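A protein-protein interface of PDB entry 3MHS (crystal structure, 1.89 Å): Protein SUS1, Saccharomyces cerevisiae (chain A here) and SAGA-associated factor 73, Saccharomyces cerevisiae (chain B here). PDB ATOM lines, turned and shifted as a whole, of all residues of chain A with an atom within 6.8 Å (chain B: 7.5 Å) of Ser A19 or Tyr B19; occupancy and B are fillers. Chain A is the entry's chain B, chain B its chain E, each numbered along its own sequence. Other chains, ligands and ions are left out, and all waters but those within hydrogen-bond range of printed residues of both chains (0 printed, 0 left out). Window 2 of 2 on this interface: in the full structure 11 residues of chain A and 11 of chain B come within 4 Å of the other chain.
Ser A19 touches just one residue of chain B: Tyr B19.
Tyr B19 touches just these residues of chain A: Tyr A15 (3.5 Å), Glu A18 (3.3 Å) and Ser A19 (3.8 Å).
Of the printed residues of chain B, Glu A18 touches Tyr B19 (3.3 Å).
Printed residues of chain B within 4 Å of Tyr A15: Val B15 and Tyr B19.
Of the printed residues of chain A, Val B15 touches Tyr A15.
Leu A24 touches none of the printed residues of chain B.
The nearest residue of chain A that does not touch Tyr B19 is Gln A14 (5.6 Å).
The nearest printed residue of chain A that does not touch Val B15 is Ile A92 (4.1 Å).
The backbone carbonyl oxygen of Tyr A15 lies within hydrogen-bond range of the side-chain hydroxyl of Ser A19 (3.1 Å).
The backbone carbonyl oxygen of Leu A16 sits at hydrogen-bond distance from the side-chain hydroxyl of Ser A19 (2.9 Å).
The side-chain amide nitrogen of Asn A21 is in hydrogen-bond range of the side-chain hydroxyl of Ser A19 (3.2 Å).
N of Ser B20 lies within hydrogen-bond range of O of Val B15.
Hydrophobic or aromatic side chains of chain B within 4 Å of the printed part of chain A: Val B15 and Tyr B19.
Along chain B the printed residues that touch a printed residue of chain A span positions 15 to 19.
Printed residues of chain A that touch a printed residue of chain B: Tyr A15, Glu A18 and Ser A19.
Hydrophobic or aromatic side chains of chain A within 4 Å of the printed part of chain B: Tyr A15.
Among the printed residues, 4 pairs touch across the chains.
Among the printed residues, no Asp or Glu carboxylate lies within 4 Å of a Lys or Arg side-chain nitrogen of the other chain.
Among the printed residues, merely in contact across the chains: Tyr A15 with Val B15 (3.3 Å), Tyr A15 with Tyr B19 (3.5 Å) and Ser A19 with Tyr B19 (3.8 Å).
The side-chain carboxylate (OE1) of Glu A18 lies close to the backbone carbonyl oxygen (O) of Tyr B19.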
ATOM      1  N   GLN A  14       8.973   3.784 -13.706  1.00  0.00           N
ATOM      2  CA  GLN A  14       7.902   4.748 -13.931  1.00  0.00           C
ATOM      3  C   GLN A  14       7.192   5.098 -12.630  1.00  0.00           C
ATOM      4  O   GLN A  14       6.946   6.293 -12.368  1.00  0.00           O
ATOM      5  CB  GLN A  14       6.890   4.220 -14.943  1.00  0.00           C
ATOM      6  CG  GLN A  14       5.750   5.190 -15.293  1.00  0.00           C
ATOM      7  CD  GLN A  14       6.040   6.036 -16.527  1.00  0.00           C
ATOM      8  OE1 GLN A  14       5.279   6.952 -16.860  1.00  0.00           O
ATOM      9  NE2 GLN A  14       7.124   5.714 -17.228  1.00  0.00           N
ATOM     10  N   TYR A  15       6.830   4.073 -11.841  1.00  0.00           N
ATOM     11  CA  TYR A  15       6.264   4.278 -10.507  1.00  0.00           C
ATOM     12  C   TYR A  15       7.164   5.095  -9.601  1.00  0.00           C
ATOM     13  O   TYR A  15       6.684   5.990  -8.895  1.00  0.00           O
ATOM     14  CB  TYR A  15       5.978   2.964  -9.766  1.00  0.00           C
ATOM     15  CG  TYR A  15       6.022   3.214  -8.275  1.00  0.00           C
ATOM     16  CD1 TYR A  15       4.974   3.871  -7.631  1.00  0.00           C
ATOM     17  CD2 TYR A  15       7.154   2.917  -7.537  1.00  0.00           C
ATOM     18  CE1 TYR A  15       5.028   4.160  -6.287  1.00  0.00           C
ATOM     19  CE2 TYR A  15       7.224   3.207  -6.191  1.00  0.00           C
ATOM     20  CZ  TYR A  15       6.155   3.826  -5.565  1.00  0.00           C
ATOM     21  OH  TYR A  15       6.229   4.118  -4.220  1.00  0.00           O
ATOM     22  N   LEU A  16       8.455   4.766  -9.561  1.00  0.00           N
ATOM     23  CA  LEU A  16       9.400   5.537  -8.754  1.00  0.00           C
ATOM     24  C   LEU A  16       9.388   7.022  -9.149  1.00  0.00           C
ATOM     25  O   LEU A  16       9.438   7.886  -8.277  1.00  0.00           O
ATOM     26  CB  LEU A  16      10.826   4.978  -8.830  1.00  0.00           C
ATOM     27  CG  LEU A  16      11.127   3.666  -8.087  1.00  0.00           C
ATOM     28  CD1 LEU A  16      12.624   3.366  -8.215  1.00  0.00           C
ATOM     29  CD2 LEU A  16      10.751   3.767  -6.623  1.00  0.00           C
ATOM     30  N   VAL A  17       9.333   7.320 -10.445  1.00  0.00           N
ATOM     31  CA  VAL A  17       9.315   8.705 -10.900  1.00  0.00           C
ATOM     32  C   VAL A  17       7.994   9.405 -10.538  1.00  0.00           C
ATOM     33  O   VAL A  17       7.986  10.539 -10.052  1.00  0.00           O
ATOM     34  CB  VAL A  17       9.549   8.829 -12.433  1.00  0.00           C
ATOM     35  CG1 VAL A  17       9.388  10.283 -12.874  1.00  0.00           C
ATOM     36  CG2 VAL A  17      10.941   8.256 -12.844  1.00  0.00           C
ATOM     37  N   GLU A  18       6.876   8.747 -10.792  1.00  0.00           N
ATOM     38  CA  GLU A  18       5.579   9.367 -10.530  1.00  0.00           C
ATOM     39  C   GLU A  18       5.361   9.609  -9.048  1.00  0.00           C
ATOM     40  O   GLU A  18       4.741  10.618  -8.667  1.00  0.00           O
ATOM     41  CB  GLU A  18       4.441   8.554 -11.161  1.00  0.00           C
ATOM     42  CG  GLU A  18       4.289   8.878 -12.646  1.00  0.00           C
ATOM     43  CD  GLU A  18       3.443   7.890 -13.414  1.00  0.00           C
ATOM     44  OE1 GLU A  18       3.252   6.741 -12.956  1.00  0.00           O
ATOM     45  OE2 GLU A  18       2.987   8.260 -14.515  1.00  0.00           O
ATOM     46  N   SER A  19       5.937   8.737  -8.213  1.00  0.00           N
ATOM     47  CA  SER A  19       5.790   8.826  -6.750  1.00  0.00           C
ATOM     48  C   SER A  19       6.637   9.911  -6.079  1.00  0.00           C
ATOM     49  O   SER A  19       6.441  10.201  -4.900  1.00  0.00           O
ATOM     50  CB  SER A  19       6.127   7.485  -6.103  1.00  0.00           C
ATOM     51  OG  SER A  19       7.515   7.218  -6.186  1.00  0.00           O
ATOM     52  N   GLY A  20       7.593  10.473  -6.814  1.00  0.00           N
ATOM     53  CA  GLY A  20       8.543  11.429  -6.263  1.00  0.00           C
ATOM     54  C   GLY A  20       9.802  10.769  -5.734  1.00  0.00           C
ATOM     55  O   GLY A  20      10.770  11.413  -5.435  1.00  0.00           O
ATOM     56  N   ASN A  21       9.815   9.449  -5.631  1.00  0.00           N
ATOM     57  CA  ASN A  21      10.919   8.782  -4.984  1.00  0.00           C
ATOM     58  C   ASN A  21      12.129   8.612  -5.865  1.00  0.00           C
ATOM     59  O   ASN A  21      13.256   8.532  -5.360  1.00  0.00           O
ATOM     60  CB  ASN A  21      10.459   7.443  -4.408  1.00  0.00           C
ATOM     61  CG  ASN A  21       9.502   7.629  -3.259  1.00  0.00           C
ATOM     62  OD1 ASN A  21       9.602   8.609  -2.504  1.00  0.00           O
ATOM     63  ND2 ASN A  21       8.522   6.754  -3.166  1.00  0.00           N
ATOM     64  N   TYR A  22      11.936   8.611  -7.177  1.00  0.00           N
ATOM     65  CA  TYR A  22      13.095   8.567  -8.087  1.00  0.00           C
ATOM     66  C   TYR A  22      13.979   9.776  -7.907  1.00  0.00           C
ATOM     67  O   TYR A  22      15.195   9.677  -7.870  1.00  0.00           O
ATOM     68  CB  TYR A  22      12.661   8.485  -9.548  1.00  0.00           C
ATOM     69  CG  TYR A  22      13.756   7.970 -10.447  1.00  0.00           C
ATOM     70  CD1 TYR A  22      13.916   6.604 -10.653  1.00  0.00           C
ATOM     71  CD2 TYR A  22      14.578   8.841 -11.154  1.00  0.00           C
ATOM     72  CE1 TYR A  22      14.890   6.124 -11.486  1.00  0.00           C
ATOM     73  CE2 TYR A  22      15.566   8.378 -12.001  1.00  0.00           C
ATOM     74  CZ  TYR A  22      15.710   7.004 -12.176  1.00  0.00           C
ATOM     75  OH  TYR A  22      16.668   6.488 -13.006  1.00  0.00           O
ATOM     76  N   GLU A  23      13.353  10.938  -7.802  1.00  0.00           N
ATOM     77  CA  GLU A  23      14.063  12.167  -7.495  1.00  0.00           C
ATOM     78  C   GLU A  23      14.826  12.060  -6.188  1.00  0.00           C
ATOM     79  O   GLU A  23      15.944  12.502  -6.113  1.00  0.00           O
ATOM     80  CB  GLU A  23      13.088  13.318  -7.370  1.00  0.00           C
ATOM     81  CG  GLU A  23      12.587  13.843  -8.667  1.00  0.00           C
ATOM     82  CD  GLU A  23      11.375  14.715  -8.460  1.00  0.00           C
ATOM     83  OE1 GLU A  23      11.543  15.911  -8.102  1.00  0.00           O
ATOM     84  OE2 GLU A  23      10.261  14.187  -8.630  1.00  0.00           O
ATOM     85  N   LEU A  24      14.200  11.559  -5.131  1.00  0.00           N
ATOM     86  CA  LEU A  24      14.885  11.450  -3.838  1.00  0.00           C
ATOM     87  C   LEU A  24      16.134  10.574  -3.952  1.00  0.00           C
ATOM     88  O   LEU A  24      17.198  10.888  -3.389  1.00  0.00           O
ATOM     89  CB  LEU A  24      13.959  10.829  -2.788  1.00  0.00           C
ATOM     90  CG  LEU A  24      12.751  11.666  -2.377  1.00  0.00           C
ATOM     91  CD1 LEU A  24      11.939  10.893  -1.319  1.00  0.00           C
ATOM     92  CD2 LEU A  24      13.232  13.047  -1.849  1.00  0.00           C
ATOM     93  N   PHE A  88      12.043   1.651  -0.975  1.00  0.00           N
ATOM     94  CA  PHE A  88      11.022   2.157  -1.883  1.00  0.00           C
ATOM     95  C   PHE A  88      10.446   1.040  -2.747  1.00  0.00           C
ATOM     96  O   PHE A  88       9.281   1.102  -3.117  1.00  0.00           O
ATOM     97  CB  PHE A  88      11.568   3.263  -2.798  1.00  0.00           C
ATOM     98  CG  PHE A  88      11.919   4.544  -2.082  1.00  0.00           C
ATOM     99  CD1 PHE A  88      11.149   5.012  -1.038  1.00  0.00           C
ATOM    100  CD2 PHE A  88      12.989   5.314  -2.510  1.00  0.00           C
ATOM    101  CE1 PHE A  88      11.463   6.185  -0.406  1.00  0.00           C
ATOM    102  CE2 PHE A  88      13.301   6.502  -1.880  1.00  0.00           C
ATOM    103  CZ  PHE A  88      12.542   6.931  -0.823  1.00  0.00           C
ATOM    104  N   GLU A  91       7.977  -1.301  -0.969  1.00  0.00           N
ATOM    105  CA  GLU A  91       6.700  -0.612  -0.839  1.00  0.00           C
ATOM    106  C   GLU A  91       5.715  -1.182  -1.857  1.00  0.00           C
ATOM    107  O   GLU A  91       4.609  -1.570  -1.490  1.00  0.00           O
ATOM    108  CB  GLU A  91       6.901   0.890  -1.090  1.00  0.00           C
ATOM    109  CG  GLU A  91       6.181   1.843  -0.140  1.00  0.00           C
ATOM    110  CD  GLU A  91       7.034   3.064   0.203  1.00  0.00           C
ATOM    111  OE1 GLU A  91       6.969   4.089  -0.508  1.00  0.00           O
ATOM    112  OE2 GLU A  91       7.809   2.993   1.172  1.00  0.00           O
ATOM    113  N   ILE A  92       6.138  -1.283  -3.121  1.00  0.00           N
ATOM    114  CA  ILE A  92       5.195  -1.546  -4.222  1.00  0.00           C
ATOM    115  C   ILE A  92       5.407  -2.794  -5.084  1.00  0.00           C
ATOM    116  O   ILE A  92       4.854  -2.898  -6.176  1.00  0.00           O
ATOM    117  CB  ILE A  92       5.063  -0.307  -5.127  1.00  0.00           C
ATOM    118  CG1 ILE A  92       6.411   0.049  -5.765  1.00  0.00           C
ATOM    119  CG2 ILE A  92       4.495   0.836  -4.318  1.00  0.00           C
ATOM    120  CD1 ILE A  92       6.517  -0.293  -7.237  1.00  0.00           C
ATOM    121  N   PRO B  13      -1.147  -4.389  -7.245  1.00  0.00           N
ATOM    122  CA  PRO B  13      -2.291  -3.854  -7.991  1.00  0.00           C
ATOM    123  C   PRO B  13      -2.768  -2.432  -7.645  1.00  0.00           C
ATOM    124  O   PRO B  13      -3.339  -1.775  -8.512  1.00  0.00           O
ATOM    125  CB  PRO B  13      -3.394  -4.873  -7.696  1.00  0.00           C
ATOM    126  CG  PRO B  13      -2.664  -6.169  -7.551  1.00  0.00           C
ATOM    127  CD  PRO B  13      -1.321  -5.828  -6.948  1.00  0.00           C
ATOM    128  N   LYS B  14      -2.566  -1.954  -6.417  1.00  0.00           N
ATOM    129  CA  LYS B  14      -3.011  -0.591  -6.069  1.00  0.00           C
ATOM    130  C   LYS B  14      -2.089   0.473  -6.668  1.00  0.00           C
ATOM    131  O   LYS B  14      -2.514   1.608  -6.931  1.00  0.00           O
ATOM    132  CB  LYS B  14      -3.099  -0.375  -4.553  1.00  0.00           C
ATOM    133  CG  LYS B  14      -3.618   1.025  -4.175  1.00  0.00           C
ATOM    134  CD  LYS B  14      -3.546   1.298  -2.679  1.00  0.00           C
ATOM    135  CE  LYS B  14      -2.264   2.023  -2.269  1.00  0.00           C
ATOM    136  NZ  LYS B  14      -2.289   3.470  -2.631  1.00  0.00           N
ATOM    137  N   VAL B  15      -0.820   0.120  -6.847  1.00  0.00           N
ATOM    138  CA  VAL B  15       0.128   1.043  -7.460  1.00  0.00           C
ATOM    139  C   VAL B  15      -0.300   1.263  -8.911  1.00  0.00           C
ATOM    140  O   VAL B  15      -0.543   2.398  -9.321  1.00  0.00           O
ATOM    141  CB  VAL B  15       1.595   0.538  -7.359  1.00  0.00           C
ATOM    142  CG1 VAL B  15       1.805  -0.739  -8.160  1.00  0.00           C
ATOM    143  CG2 VAL B  15       2.556   1.614  -7.823  1.00  0.00           C
ATOM    144  N   ILE B  16      -0.473   0.167  -9.652  1.00  0.00           N
ATOM    145  CA  ILE B  16      -0.961   0.227 -11.032  1.00  0.00           C
ATOM    146  C   ILE B  16      -2.263   1.026 -11.103  1.00  0.00           C
ATOM    147  O   ILE B  16      -2.510   1.744 -12.069  1.00  0.00           O
ATOM    148  CB  ILE B  16      -1.217  -1.187 -11.623  1.00  0.00           C
ATOM    149  CG1 ILE B  16       0.077  -2.010 -11.659  1.00  0.00           C
ATOM    150  CG2 ILE B  16      -1.800  -1.084 -13.031  1.00  0.00           C
ATOM    151  CD1 ILE B  16      -0.075  -3.366 -12.330  1.00  0.00           C
ATOM    152  N   GLU B  17      -3.080   0.915 -10.063  1.00  0.00           N
ATOM    153  CA  GLU B  17      -4.416   1.494 -10.082  1.00  0.00           C
ATOM    154  C   GLU B  17      -4.367   2.994 -10.318  1.00  0.00           C
ATOM    155  O   GLU B  17      -5.175   3.539 -11.065  1.00  0.00           O
ATOM    156  CB  GLU B  17      -5.159   1.202  -8.770  1.00  0.00           C
ATOM    157  CG  GLU B  17      -6.676   1.246  -8.893  1.00  0.00           C
ATOM    158  CD  GLU B  17      -7.248  -0.003  -9.547  1.00  0.00           C
ATOM    159  OE1 GLU B  17      -6.803  -0.358 -10.658  1.00  0.00           O
ATOM    160  OE2 GLU B  17      -8.139  -0.636  -8.947  1.00  0.00           O
ATOM    161  N   GLU B  18      -3.428   3.664  -9.669  1.00  0.00           N
ATOM    162  CA  GLU B  18      -3.355   5.111  -9.767  1.00  0.00           C
ATOM    163  C   GLU B  18      -2.032   5.608 -10.377  1.00  0.00           C
ATOM    164  O   GLU B  18      -1.957   6.749 -10.826  1.00  0.00           O
ATOM    165  CB  GLU B  18      -3.703   5.726  -8.399  1.00  0.00           C
ATOM    166  CG  GLU B  18      -3.068   7.065  -8.049  1.00  0.00           C
ATOM    167  CD  GLU B  18      -2.165   6.974  -6.830  1.00  0.00           C
ATOM    168  OE1 GLU B  18      -2.048   5.866  -6.254  1.00  0.00           O
ATOM    169  OE2 GLU B  18      -1.583   8.012  -6.440  1.00  0.00           O
ATOM    170  N   TYR B  19      -1.029   4.729 -10.469  1.00  0.00           N
ATOM    171  CA  TYR B  19       0.265   5.056 -11.112  1.00  0.00           C
ATOM    172  C   TYR B  19       0.446   4.358 -12.467  1.00  0.00           C
ATOM    173  O   TYR B  19       0.450   5.008 -13.513  1.00  0.00           O
ATOM    174  CB  TYR B  19       1.454   4.644 -10.225  1.00  0.00           C
ATOM    175  CG  TYR B  19       1.673   5.481  -8.987  1.00  0.00           C
ATOM    176  CD1 TYR B  19       1.971   6.831  -9.081  1.00  0.00           C
ATOM    177  CD2 TYR B  19       1.632   4.905  -7.722  1.00  0.00           C
ATOM    178  CE1 TYR B  19       2.181   7.596  -7.948  1.00  0.00           C
ATOM    179  CE2 TYR B  19       1.848   5.664  -6.588  1.00  0.00           C
ATOM    180  CZ  TYR B  19       2.123   7.006  -6.710  1.00  0.00           C
ATOM    181  OH  TYR B  19       2.329   7.762  -5.586  1.00  0.00           O
ATOM    182  N   SER B  20       0.620   3.035 -12.418  1.00  0.00           N
ATOM    183  CA  SER B  20       0.997   2.199 -13.569  1.00  0.00           C
ATOM    184  C   SER B  20       2.524   2.078 -13.642  1.00  0.00           C
ATOM    185  O   SER B  20       3.192   1.848 -12.629  1.00  0.00           O
ATOM    186  CB  SER B  20       0.434   2.743 -14.890  1.00  0.00           C
ATOM    187  OG  SER B  20      -0.884   3.240 -14.721  1.00  0.00           O
